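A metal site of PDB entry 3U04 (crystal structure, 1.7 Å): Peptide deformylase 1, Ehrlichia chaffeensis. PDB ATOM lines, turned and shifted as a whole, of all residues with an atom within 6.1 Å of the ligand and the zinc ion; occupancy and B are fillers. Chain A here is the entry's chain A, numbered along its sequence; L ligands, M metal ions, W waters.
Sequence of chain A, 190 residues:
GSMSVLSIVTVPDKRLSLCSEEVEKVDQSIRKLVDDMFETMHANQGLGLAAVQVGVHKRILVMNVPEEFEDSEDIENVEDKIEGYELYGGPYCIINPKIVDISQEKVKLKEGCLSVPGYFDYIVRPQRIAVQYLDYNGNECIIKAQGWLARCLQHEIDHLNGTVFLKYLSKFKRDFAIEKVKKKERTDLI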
ATOM      1  N   ASN A  44     -26.901  19.112  32.447  1.00  0.00           N
ATOM      2  CA  ASN A  44     -26.011  18.197  31.741  1.00  0.00           C
ATOM      3  C   ASN A  44     -24.545  18.621  31.755  1.00  0.00           C
ATOM      4  O   ASN A  44     -23.718  17.991  31.099  1.00  0.00           O
ATOM      5  CB  ASN A  44     -26.505  18.023  30.293  1.00  0.00           C
ATOM      6  CG  ASN A  44     -27.617  17.028  30.201  1.00  0.00           C
ATOM      7  OD1 ASN A  44     -27.392  15.814  30.349  1.00  0.00           O
ATOM      8  ND2 ASN A  44     -28.859  17.507  30.007  1.00  0.00           N
ATOM      9  N   GLN A  45     -24.233  19.660  32.526  1.00  0.00           N
ATOM     10  CA  GLN A  45     -22.869  20.166  32.645  1.00  0.00           C
ATOM     11  C   GLN A  45     -22.276  20.600  31.315  1.00  0.00           C
ATOM     12  O   GLN A  45     -21.093  20.366  31.081  1.00  0.00           O
ATOM     13  CB  GLN A  45     -21.954  19.094  33.308  1.00  0.00           C
ATOM     14  CG  GLN A  45     -22.443  18.692  34.678  1.00  0.00           C
ATOM     15  CD  GLN A  45     -22.283  19.823  35.681  1.00  0.00           C
ATOM     16  OE1 GLN A  45     -21.226  20.457  35.749  1.00  0.00           O
ATOM     17  NE2 GLN A  45     -23.347  20.104  36.433  1.00  0.00           N
ATOM     18  N   GLY A  46     -23.118  21.167  30.455  1.00  0.00           N
ATOM     19  CA  GLY A  46     -22.678  21.627  29.118  1.00  0.00           C
ATOM     20  C   GLY A  46     -22.239  23.076  29.059  1.00  0.00           C
ATOM     21  O   GLY A  46     -22.643  23.922  29.873  1.00  0.00           O
ATOM     22  N   LEU A  47     -21.451  23.395  28.029  1.00  0.00           N
ATOM     23  CA  LEU A  47     -21.070  24.761  27.707  1.00  0.00           C
ATOM     24  C   LEU A  47     -22.073  25.454  26.748  1.00  0.00           C
ATOM     25  O   LEU A  47     -22.064  26.667  26.579  1.00  0.00           O
ATOM     26  CB  LEU A  47     -19.707  24.719  27.025  1.00  0.00           C
ATOM     27  CG  LEU A  47     -18.469  24.358  27.829  1.00  0.00           C
ATOM     28  CD1 LEU A  47     -17.289  24.147  26.851  1.00  0.00           C
ATOM     29  CD2 LEU A  47     -18.203  25.472  28.819  1.00  0.00           C
ATOM     30  N   GLY A  48     -22.884  24.651  26.069  1.00  0.00           N
ATOM     31  CA  GLY A  48     -23.865  25.157  25.133  1.00  0.00           C
ATOM     32  C   GLY A  48     -24.878  24.079  24.832  1.00  0.00           C
ATOM     33  O   GLY A  48     -24.723  22.949  25.299  1.00  0.00           O
ATOM     34  N   LEU A  49     -25.882  24.429  24.021  1.00  0.00           N
ATOM     35  CA  LEU A  49     -26.897  23.474  23.610  1.00  0.00           C
ATOM     36  C   LEU A  49     -27.658  24.041  22.432  1.00  0.00           C
ATOM     37  O   LEU A  49     -27.897  25.244  22.364  1.00  0.00           O
ATOM     38  CB  LEU A  49     -27.883  23.195  24.778  1.00  0.00           C
ATOM     39  CG  LEU A  49     -28.836  22.007  24.665  1.00  0.00           C
ATOM     40  CD1 LEU A  49     -28.069  20.694  24.785  1.00  0.00           C
ATOM     41  CD2 LEU A  49     -29.907  22.091  25.758  1.00  0.00           C
ATOM     42  N   ALA A  50     -27.988  23.177  21.480  1.00  0.00           N
ATOM     43  CA  ALA A  50     -28.776  23.567  20.328  1.00  0.00           C
ATOM     44  C   ALA A  50     -30.170  22.999  20.431  1.00  0.00           C
ATOM     45  O   ALA A  50     -30.355  21.926  20.986  1.00  0.00           O
ATOM     46  CB  ALA A  50     -28.098  23.088  19.034  1.00  0.00           C
ATOM     47  N   GLN A  53     -31.065  19.314  19.666  1.00  0.00           N
ATOM     48  CA  GLN A  53     -30.654  18.365  20.681  1.00  0.00           C
ATOM     49  C   GLN A  53     -31.753  18.119  21.704  1.00  0.00           C
ATOM     50  O   GLN A  53     -31.645  17.135  22.447  1.00  0.00           O
ATOM     51  CB  GLN A  53     -29.396  18.862  21.390  1.00  0.00           C
ATOM     52  CG  GLN A  53     -28.187  18.938  20.491  1.00  0.00           C
ATOM     53  CD  GLN A  53     -26.973  19.352  21.261  1.00  0.00           C
ATOM     54  OE1 GLN A  53     -26.765  20.537  21.479  1.00  0.00           O
ATOM     55  NE2 GLN A  53     -26.211  18.372  21.776  1.00  0.00           N
ATOM     56  N   LEU A 109      -8.710  21.414  19.197  1.00  0.00           N
ATOM     57  CA  LEU A 109      -9.146  21.306  20.595  1.00  0.00           C
ATOM     58  C   LEU A 109      -9.992  20.039  20.776  1.00  0.00           C
ATOM     59  O   LEU A 109     -10.582  19.530  19.828  1.00  0.00           O
ATOM     60  CB  LEU A 109      -9.980  22.509  20.981  1.00  0.00           C
ATOM     61  CG  LEU A 109      -9.263  23.861  21.091  1.00  0.00           C
ATOM     62  CD1 LEU A 109     -10.311  24.998  21.253  1.00  0.00           C
ATOM     63  CD2 LEU A 109      -8.234  23.862  22.211  1.00  0.00           C
ATOM     64  N   LYS A 110     -10.030  19.539  21.994  1.00  0.00           N
ATOM     65  CA  LYS A 110     -10.787  18.350  22.325  1.00  0.00           C
ATOM     66  C   LYS A 110     -12.253  18.746  22.525  1.00  0.00           C
ATOM     67  O   LYS A 110     -12.542  19.747  23.212  1.00  0.00           O
ATOM     68  CB  LYS A 110     -10.257  17.738  23.605  1.00  0.00           C
ATOM     69  CG  LYS A 110     -10.917  16.403  23.900  1.00  0.00           C
ATOM     70  CD  LYS A 110     -10.260  15.650  25.039  1.00  0.00           C
ATOM     71  CE  LYS A 110     -10.826  16.020  26.379  1.00  0.00           C
ATOM     72  NZ  LYS A 110     -10.278  15.107  27.434  1.00  0.00           N
ATOM     73  N   GLU A 111     -13.139  17.970  21.925  1.00  0.00           N
ATOM     74  CA  GLU A 111     -14.591  18.190  22.075  1.00  0.00           C
ATOM     75  C   GLU A 111     -15.304  16.940  22.482  1.00  0.00           C
ATOM     76  O   GLU A 111     -14.946  15.852  22.070  1.00  0.00           O
ATOM     77  CB  GLU A 111     -15.208  18.611  20.732  1.00  0.00           C
ATOM     78  CG  GLU A 111     -14.701  19.884  20.196  1.00  0.00           C
ATOM     79  CD  GLU A 111     -15.430  20.384  18.961  1.00  0.00           C
ATOM     80  OE1 GLU A 111     -16.655  20.058  18.745  1.00  0.00           O
ATOM     81  OE2 GLU A 111     -14.750  21.111  18.232  1.00  0.00           O
ATOM     82  N   GLY A 112     -16.388  17.123  23.249  1.00  0.00           N
ATOM     83  CA  GLY A 112     -17.412  16.121  23.358  1.00  0.00           C
ATOM     84  C   GLY A 112     -18.728  16.777  23.050  1.00  0.00           C
ATOM     85  O   GLY A 112     -18.792  17.975  22.725  1.00  0.00           O
ATOM     86  N   CYS A 113     -19.776  15.971  23.113  1.00  0.00           N
ATOM     87  CA  CYS A 113     -21.131  16.437  22.750  1.00  0.00           C
ATOM     88  C   CYS A 113     -22.145  15.714  23.579  1.00  0.00           C
ATOM     89  O   CYS A 113     -22.053  14.471  23.737  1.00  0.00           O
ATOM     90  CB  CYS A 113     -21.411  16.108  21.289  1.00  0.00           C
ATOM     91  SG  CYS A 113     -22.975  16.654  20.574  1.00  0.00           S
ATOM     92  N   LEU A 114     -23.182  16.424  24.009  1.00  0.00           N
ATOM     93  CA  LEU A 114     -24.249  15.758  24.765  1.00  0.00           C
ATOM     94  C   LEU A 114     -25.028  14.704  23.963  1.00  0.00           C
ATOM     95  O   LEU A 114     -25.597  13.760  24.540  1.00  0.00           O
ATOM     96  CB  LEU A 114     -25.222  16.803  25.371  1.00  0.00           C
ATOM     97  CG  LEU A 114     -24.523  17.767  26.351  1.00  0.00           C
ATOM     98  CD1 LEU A 114     -25.503  18.819  26.819  1.00  0.00           C
ATOM     99  CD2 LEU A 114     -23.975  17.023  27.549  1.00  0.00           C
ATOM    100  N   SER A 115     -25.023  14.835  22.644  1.00  0.00           N
ATOM    101  CA  SER A 115     -25.669  13.891  21.740  1.00  0.00           C
ATOM    102  C   SER A 115     -24.770  12.709  21.364  1.00  0.00           C
ATOM    103  O   SER A 115     -25.205  11.786  20.685  1.00  0.00           O
ATOM    104  CB  SER A 115     -26.117  14.611  20.468  1.00  0.00           C
ATOM    105  OG  SER A 115     -27.014  15.623  20.796  1.00  0.00           O
ATOM    106  N   TYR A 119     -18.030  10.187  24.474  1.00  0.00           N
ATOM    107  CA  TYR A 119     -17.014  10.102  23.417  1.00  0.00           C
ATOM    108  C   TYR A 119     -16.383  11.466  23.240  1.00  0.00           C
ATOM    109  O   TYR A 119     -17.090  12.454  23.015  1.00  0.00           O
ATOM    110  CB  TYR A 119     -17.613   9.619  22.064  1.00  0.00           C
ATOM    111  CG  TYR A 119     -16.561   9.376  21.042  1.00  0.00           C
ATOM    112  CD1 TYR A 119     -15.869   8.192  21.017  1.00  0.00           C
ATOM    113  CD2 TYR A 119     -16.231  10.351  20.099  1.00  0.00           C
ATOM    114  CE1 TYR A 119     -14.848   7.978  20.104  1.00  0.00           C
ATOM    115  CE2 TYR A 119     -15.210  10.137  19.185  1.00  0.00           C
ATOM    116  CZ  TYR A 119     -14.530   8.949  19.186  1.00  0.00           C
ATOM    117  OH  TYR A 119     -13.497   8.731  18.301  1.00  0.00           O
ATOM    118  N   PHE A 120     -15.064  11.513  23.311  1.00  0.00           N
ATOM    119  CA  PHE A 120     -14.314  12.762  23.064  1.00  0.00           C
ATOM    120  C   PHE A 120     -13.308  12.587  21.935  1.00  0.00           C
ATOM    121  O   PHE A 120     -12.720  11.532  21.783  1.00  0.00           O
ATOM    122  CB  PHE A 120     -13.568  13.194  24.316  1.00  0.00           C
ATOM    123  CG  PHE A 120     -14.445  13.576  25.451  1.00  0.00           C
ATOM    124  CD1 PHE A 120     -14.998  12.583  26.267  1.00  0.00           C
ATOM    125  CD2 PHE A 120     -14.745  14.922  25.706  1.00  0.00           C
ATOM    126  CE1 PHE A 120     -15.845  12.938  27.326  1.00  0.00           C
ATOM    127  CE2 PHE A 120     -15.577  15.261  26.754  1.00  0.00           C
ATOM    128  CZ  PHE A 120     -16.124  14.270  27.557  1.00  0.00           C
ATOM    129  N   ARG A 125     -10.843  23.649  14.095  1.00  0.00           N
ATOM    130  CA  ARG A 125     -11.783  24.700  13.717  1.00  0.00           C
ATOM    131  C   ARG A 125     -11.093  26.066  13.736  1.00  0.00           C
ATOM    132  O   ARG A 125     -10.134  26.243  14.467  1.00  0.00           O
ATOM    133  CB  ARG A 125     -12.964  24.800  14.688  1.00  0.00           C
ATOM    134  CG  ARG A 125     -13.759  23.493  14.896  1.00  0.00           C
ATOM    135  CD  ARG A 125     -14.966  23.833  15.705  1.00  0.00           C
ATOM    136  NE  ARG A 125     -15.747  22.665  16.155  1.00  0.00           N
ATOM    137  CZ  ARG A 125     -16.805  22.159  15.510  1.00  0.00           C
ATOM    138  NH1 ARG A 125     -17.310  22.711  14.416  1.00  0.00           N
ATOM    139  NH2 ARG A 125     -17.405  21.097  16.047  1.00  0.00           N
ATOM    140  N   TRP A 148     -12.390  29.207  23.904  1.00  0.00           N
ATOM    141  CA  TRP A 148     -13.456  28.246  24.078  1.00  0.00           C
ATOM    142  C   TRP A 148     -14.822  28.775  23.726  1.00  0.00           C
ATOM    143  O   TRP A 148     -15.707  28.000  23.389  1.00  0.00           O
ATOM    144  CB  TRP A 148     -13.467  27.687  25.491  1.00  0.00           C
ATOM    145  CG  TRP A 148     -12.335  26.727  25.745  1.00  0.00           C
ATOM    146  CD1 TRP A 148     -11.141  26.948  26.446  1.00  0.00           C
ATOM    147  CD2 TRP A 148     -12.222  25.370  25.246  1.00  0.00           C
ATOM    148  NE1 TRP A 148     -10.345  25.826  26.433  1.00  0.00           N
ATOM    149  CE2 TRP A 148     -10.954  24.841  25.740  1.00  0.00           C
ATOM    150  CE3 TRP A 148     -13.036  24.550  24.508  1.00  0.00           C
ATOM    151  CZ2 TRP A 148     -10.540  23.536  25.466  1.00  0.00           C
ATOM    152  CZ3 TRP A 148     -12.620  23.246  24.244  1.00  0.00           C
ATOM    153  CH2 TRP A 148     -11.402  22.758  24.712  1.00  0.00           C
ATOM    154  N   ARG A 151     -15.077  28.241  20.051  1.00  0.00           N
ATOM    155  CA  ARG A 151     -15.178  26.796  19.839  1.00  0.00           C
ATOM    156  C   ARG A 151     -16.589  26.255  20.089  1.00  0.00           C
ATOM    157  O   ARG A 151     -17.156  25.567  19.268  1.00  0.00           O
ATOM    158  CB  ARG A 151     -14.156  26.063  20.739  1.00  0.00           C
ATOM    159  CG  ARG A 151     -14.248  24.525  20.693  1.00  0.00           C
ATOM    160  CD  ARG A 151     -14.236  23.943  19.314  1.00  0.00           C
ATOM    161  NE  ARG A 151     -12.991  24.353  18.608  1.00  0.00           N
ATOM    162  CZ  ARG A 151     -12.071  23.536  18.105  1.00  0.00           C
ATOM    163  NH1 ARG A 151     -12.210  22.207  18.153  1.00  0.00           N
ATOM    164  NH2 ARG A 151     -10.979  24.098  17.544  1.00  0.00           N
ATOM    165  N   CYS A 152     -17.173  26.641  21.208  1.00  0.00           N
ATOM    166  CA  CYS A 152     -18.533  26.253  21.528  1.00  0.00           C
ATOM    167  C   CYS A 152     -19.524  26.744  20.482  1.00  0.00           C
ATOM    168  O   CYS A 152     -20.402  26.000  20.073  1.00  0.00           O
ATOM    169  CB  CYS A 152     -18.903  26.731  22.909  1.00  0.00           C
ATOM    170  SG  CYS A 152     -20.587  26.272  23.426  1.00  0.00           S
ATOM    171  N   HIS A 155     -19.458  24.688  17.344  1.00  0.00           N
ATOM    172  CA  HIS A 155     -20.029  23.359  17.603  1.00  0.00           C
ATOM    173  C   HIS A 155     -21.532  23.476  17.610  1.00  0.00           C
ATOM    174  O   HIS A 155     -22.223  22.677  16.951  1.00  0.00           O
ATOM    175  CB  HIS A 155     -19.452  22.838  18.904  1.00  0.00           C
ATOM    176  CG  HIS A 155     -20.036  21.545  19.391  1.00  0.00           C
ATOM    177  ND1 HIS A 155     -19.276  20.445  19.563  1.00  0.00           N
ATOM    178  CD2 HIS A 155     -21.309  21.209  19.825  1.00  0.00           C
ATOM    179  CE1 HIS A 155     -20.050  19.439  20.039  1.00  0.00           C
ATOM    180  NE2 HIS A 155     -21.289  19.896  20.208  1.00  0.00           N
ATOM    181  N   GLU A 156     -22.079  24.524  18.217  1.00  0.00           N
ATOM    182  CA  GLU A 156     -23.552  24.695  18.309  1.00  0.00           C
ATOM    183  C   GLU A 156     -24.129  25.053  16.906  1.00  0.00           C
ATOM    184  O   GLU A 156     -25.167  24.497  16.478  1.00  0.00           O
ATOM    185  CB  GLU A 156     -23.952  25.772  19.326  1.00  0.00           C
ATOM    186  CG  GLU A 156     -23.517  25.519  20.786  1.00  0.00           C
ATOM    187  CD  GLU A 156     -23.870  24.154  21.344  1.00  0.00           C
ATOM    188  OE1 GLU A 156     -24.805  23.507  20.834  1.00  0.00           O
ATOM    189  OE2 GLU A 156     -23.155  23.734  22.290  1.00  0.00           O
ATOM    190  N   HIS A 159     -24.704  22.070  14.805  1.00  0.00           N
ATOM    191  CA  HIS A 159     -25.903  21.301  15.101  1.00  0.00           C
ATOM    192  C   HIS A 159     -27.110  21.848  14.354  1.00  0.00           C
ATOM    193  O   HIS A 159     -27.997  21.078  13.953  1.00  0.00           O
ATOM    194  CB  HIS A 159     -26.234  21.340  16.587  1.00  0.00           C
ATOM    195  CG  HIS A 159     -25.506  20.372  17.436  1.00  0.00           C
ATOM    196  ND1 HIS A 159     -25.597  19.014  17.266  1.00  0.00           N
ATOM    197  CD2 HIS A 159     -24.760  20.563  18.581  1.00  0.00           C
ATOM    198  CE1 HIS A 159     -24.900  18.398  18.239  1.00  0.00           C
ATOM    199  NE2 HIS A 159     -24.374  19.342  19.036  1.00  0.00           N
ATOM    200  N   PHE A 165     -20.180  16.518  15.586  1.00  0.00           N
ATOM    201  CA  PHE A 165     -18.726  16.680  15.469  1.00  0.00           C
ATOM    202  C   PHE A 165     -18.037  15.428  14.942  1.00  0.00           C
ATOM    203  O   PHE A 165     -16.930  15.504  14.461  1.00  0.00           O
ATOM    204  CB  PHE A 165     -18.061  17.178  16.770  1.00  0.00           C
ATOM    205  CG  PHE A 165     -17.835  16.111  17.828  1.00  0.00           C
ATOM    206  CD1 PHE A 165     -18.903  15.573  18.515  1.00  0.00           C
ATOM    207  CD2 PHE A 165     -16.555  15.698  18.178  1.00  0.00           C
ATOM    208  CE1 PHE A 165     -18.711  14.597  19.530  1.00  0.00           C
ATOM    209  CE2 PHE A 165     -16.360  14.709  19.153  1.00  0.00           C
ATOM    210  CZ  PHE A 165     -17.437  14.175  19.820  1.00  0.00           C
HETATM  211  C1  LIG L   1     -22.421  20.493  24.558  1.00  0.00           C
HETATM  212  C2  LIG L   1     -23.127  20.101  23.308  1.00  0.00           C
HETATM  213  O1  LIG L   1     -23.194  18.958  22.800  1.00  0.00           O
HETATM  214  N1  LIG L   1     -23.621  21.129  22.637  1.00  0.00           N
HETATM  215  O2  LIG L   1     -24.083  20.888  21.385  1.00  0.00           O
HETATM  216  C3  LIG L   1     -20.910  20.682  24.314  1.00  0.00           C
HETATM  217  C4  LIG L   1     -20.216  20.460  25.604  1.00  0.00           C
HETATM  218  O3  LIG L   1     -20.522  21.123  26.590  1.00  0.00           O
HETATM  219  C5  LIG L   1     -20.585  22.086  23.851  1.00  0.00           C
HETATM  220  C6  LIG L   1     -19.072  22.389  23.752  1.00  0.00           C
HETATM  221  C7  LIG L   1     -18.589  22.129  22.347  1.00  0.00           C
HETATM  222  C8  LIG L   1     -17.119  22.448  22.023  1.00  0.00           C
HETATM  223  C9  LIG L   1     -16.140  22.349  23.168  1.00  0.00           C
HETATM  224  N2  LIG L   1     -19.254  19.540  25.598  1.00  0.00           N
HETATM  225  C10 LIG L   1     -18.342  19.353  26.737  1.00  0.00           C
HETATM  226  C11 LIG L   1     -18.619  18.054  27.493  1.00  0.00           C
HETATM  227  C12 LIG L   1     -19.908  18.177  28.318  1.00  0.00           C
HETATM  228  C13 LIG L   1     -18.784  16.839  26.594  1.00  0.00           C
HETATM  229  C14 LIG L   1     -16.912  19.515  26.236  1.00  0.00           C
HETATM  230  O4  LIG L   1     -16.653  19.150  25.104  1.00  0.00           O
HETATM  231  N3  LIG L   1     -15.994  20.132  27.011  1.00  0.00           N
HETATM  232  C15 LIG L   1     -14.605  20.357  26.570  1.00  0.00           C
HETATM  233  C16 LIG L   1     -16.229  20.716  28.354  1.00  0.00           C
HETATM  234  C17 LIG L   1     -14.864  21.189  28.849  1.00  0.00           C
HETATM  235  C18 LIG L   1     -14.005  21.323  27.598  1.00  0.00           C
HETATM  236  C19 LIG L   1     -13.826  19.056  26.515  1.00  0.00           C
HETATM  237  O5  LIG L   1     -12.481  19.336  26.054  1.00  0.00           O
HETATM  238 ZN    ZN M   1     -23.081  18.982  20.693  1.00  0.00          ZN
HETATM  239  O   HOH W   1      -9.693  20.089  26.553  1.00  0.00           O
HETATM  240  O   HOH W   2     -21.551  17.610  17.884  1.00  0.00           O
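Gln 53 touches the zinc ion. The nearest printed residue that does not touch the zinc ion is Leu 114 (4.2 Å).
Gln 45 touches the ligand (O to C12, 3.7 Å). Gly 46 touches the ligand (CA to O3, 3.4 Å). C of Glu 111 touches O4 of the ligand, at 3.7 Å. CE2 of Phe 120 touches C13 of the ligand, at 3.6 Å. CZ3 of Trp 148 touches C9 of the ligand, at 3.8 Å. Arg 151 touches the ligand (CG to C8, 3.8 Å). Hydrophobic or aromatic side chains within 4 Å of the ligand: Leu 47, Leu 114, Phe 120, Trp 148, His 155 and His 159. Of the 25 residues printed, 16 come within 4 Å of the ligand.
N2 of the ligand sits at hydrogen-bond distance from O of Gly 112 (3.3 Å). OE1 of Gln 53 lies within hydrogen-bond range of N1 of the ligand, 3.4 Å away. A nitrogen (N1) of the ligand lies within hydrogen-bond range of the side-chain carboxylate of Glu 156 (2.7 Å). An oxygen (O3) of the ligand sits at hydrogen-bond distance from the backbone NH of Leu 47 (2.8 Å). O of Gly 48 lies within hydrogen-bond range of N1 of the ligand. An oxygen (O4) of the ligand sits at hydrogen-bond distance from the backbone NH of Gly 112 (2.8 Å). The backbone NH (N) of Leu 114 sits close to an oxygen (O1) of the ligand (2.8 Å). An oxygen (O5) of the ligand is in hydrogen-bond range of the backbone carbonyl oxygen (O) of Lys 110 (2.9 Å).
The side-chain amide nitrogen of Gln 53 is in hydrogen-bond range of the side-chain hydroxyl of Ser 115 (3.0 Å). The side-chain carboxylate (OE1) of Glu 156 is in hydrogen-bond range of the backbone NH (N) of Ala 50, at 3.3 Å. The side-chain sulfur (SG) of Cys 152 lies within hydrogen-bond range of the side-chain carboxylate (OE2) of Glu 156. The backbone NH (N) of Leu 49 is in hydrogen-bond range of the side-chain carboxylate (OE2) of Glu 156, 3.3 Å away. A ring nitrogen (NE2) of His 159 sits close to the side-chain amide nitrogen of Gln 53 (3.4 Å). The side-chain amide oxygen of Gln 53 is in hydrogen-bond range of the backbone NH of Ala 50. A ring nitrogen (ND1) of His 155 sits at hydrogen-bond distance from the side-chain carboxylate (OE1) of Glu 111 (2.8 Å). OE2 of Glu 111 is in salt-bridge range of NE of Arg 125, 2.8 Å away.
The zinc ion is bound by a ring nitrogen (NE2) of His 155 (2.1 Å), an oxygen (O1) of the ligand (2.1 Å), a ring nitrogen (NE2) of His 159 (2.1 Å), an oxygen (O2) of the ligand (2.3 Å) and the side-chain sulfur (SG) of Cys 113 (2.3 Å).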
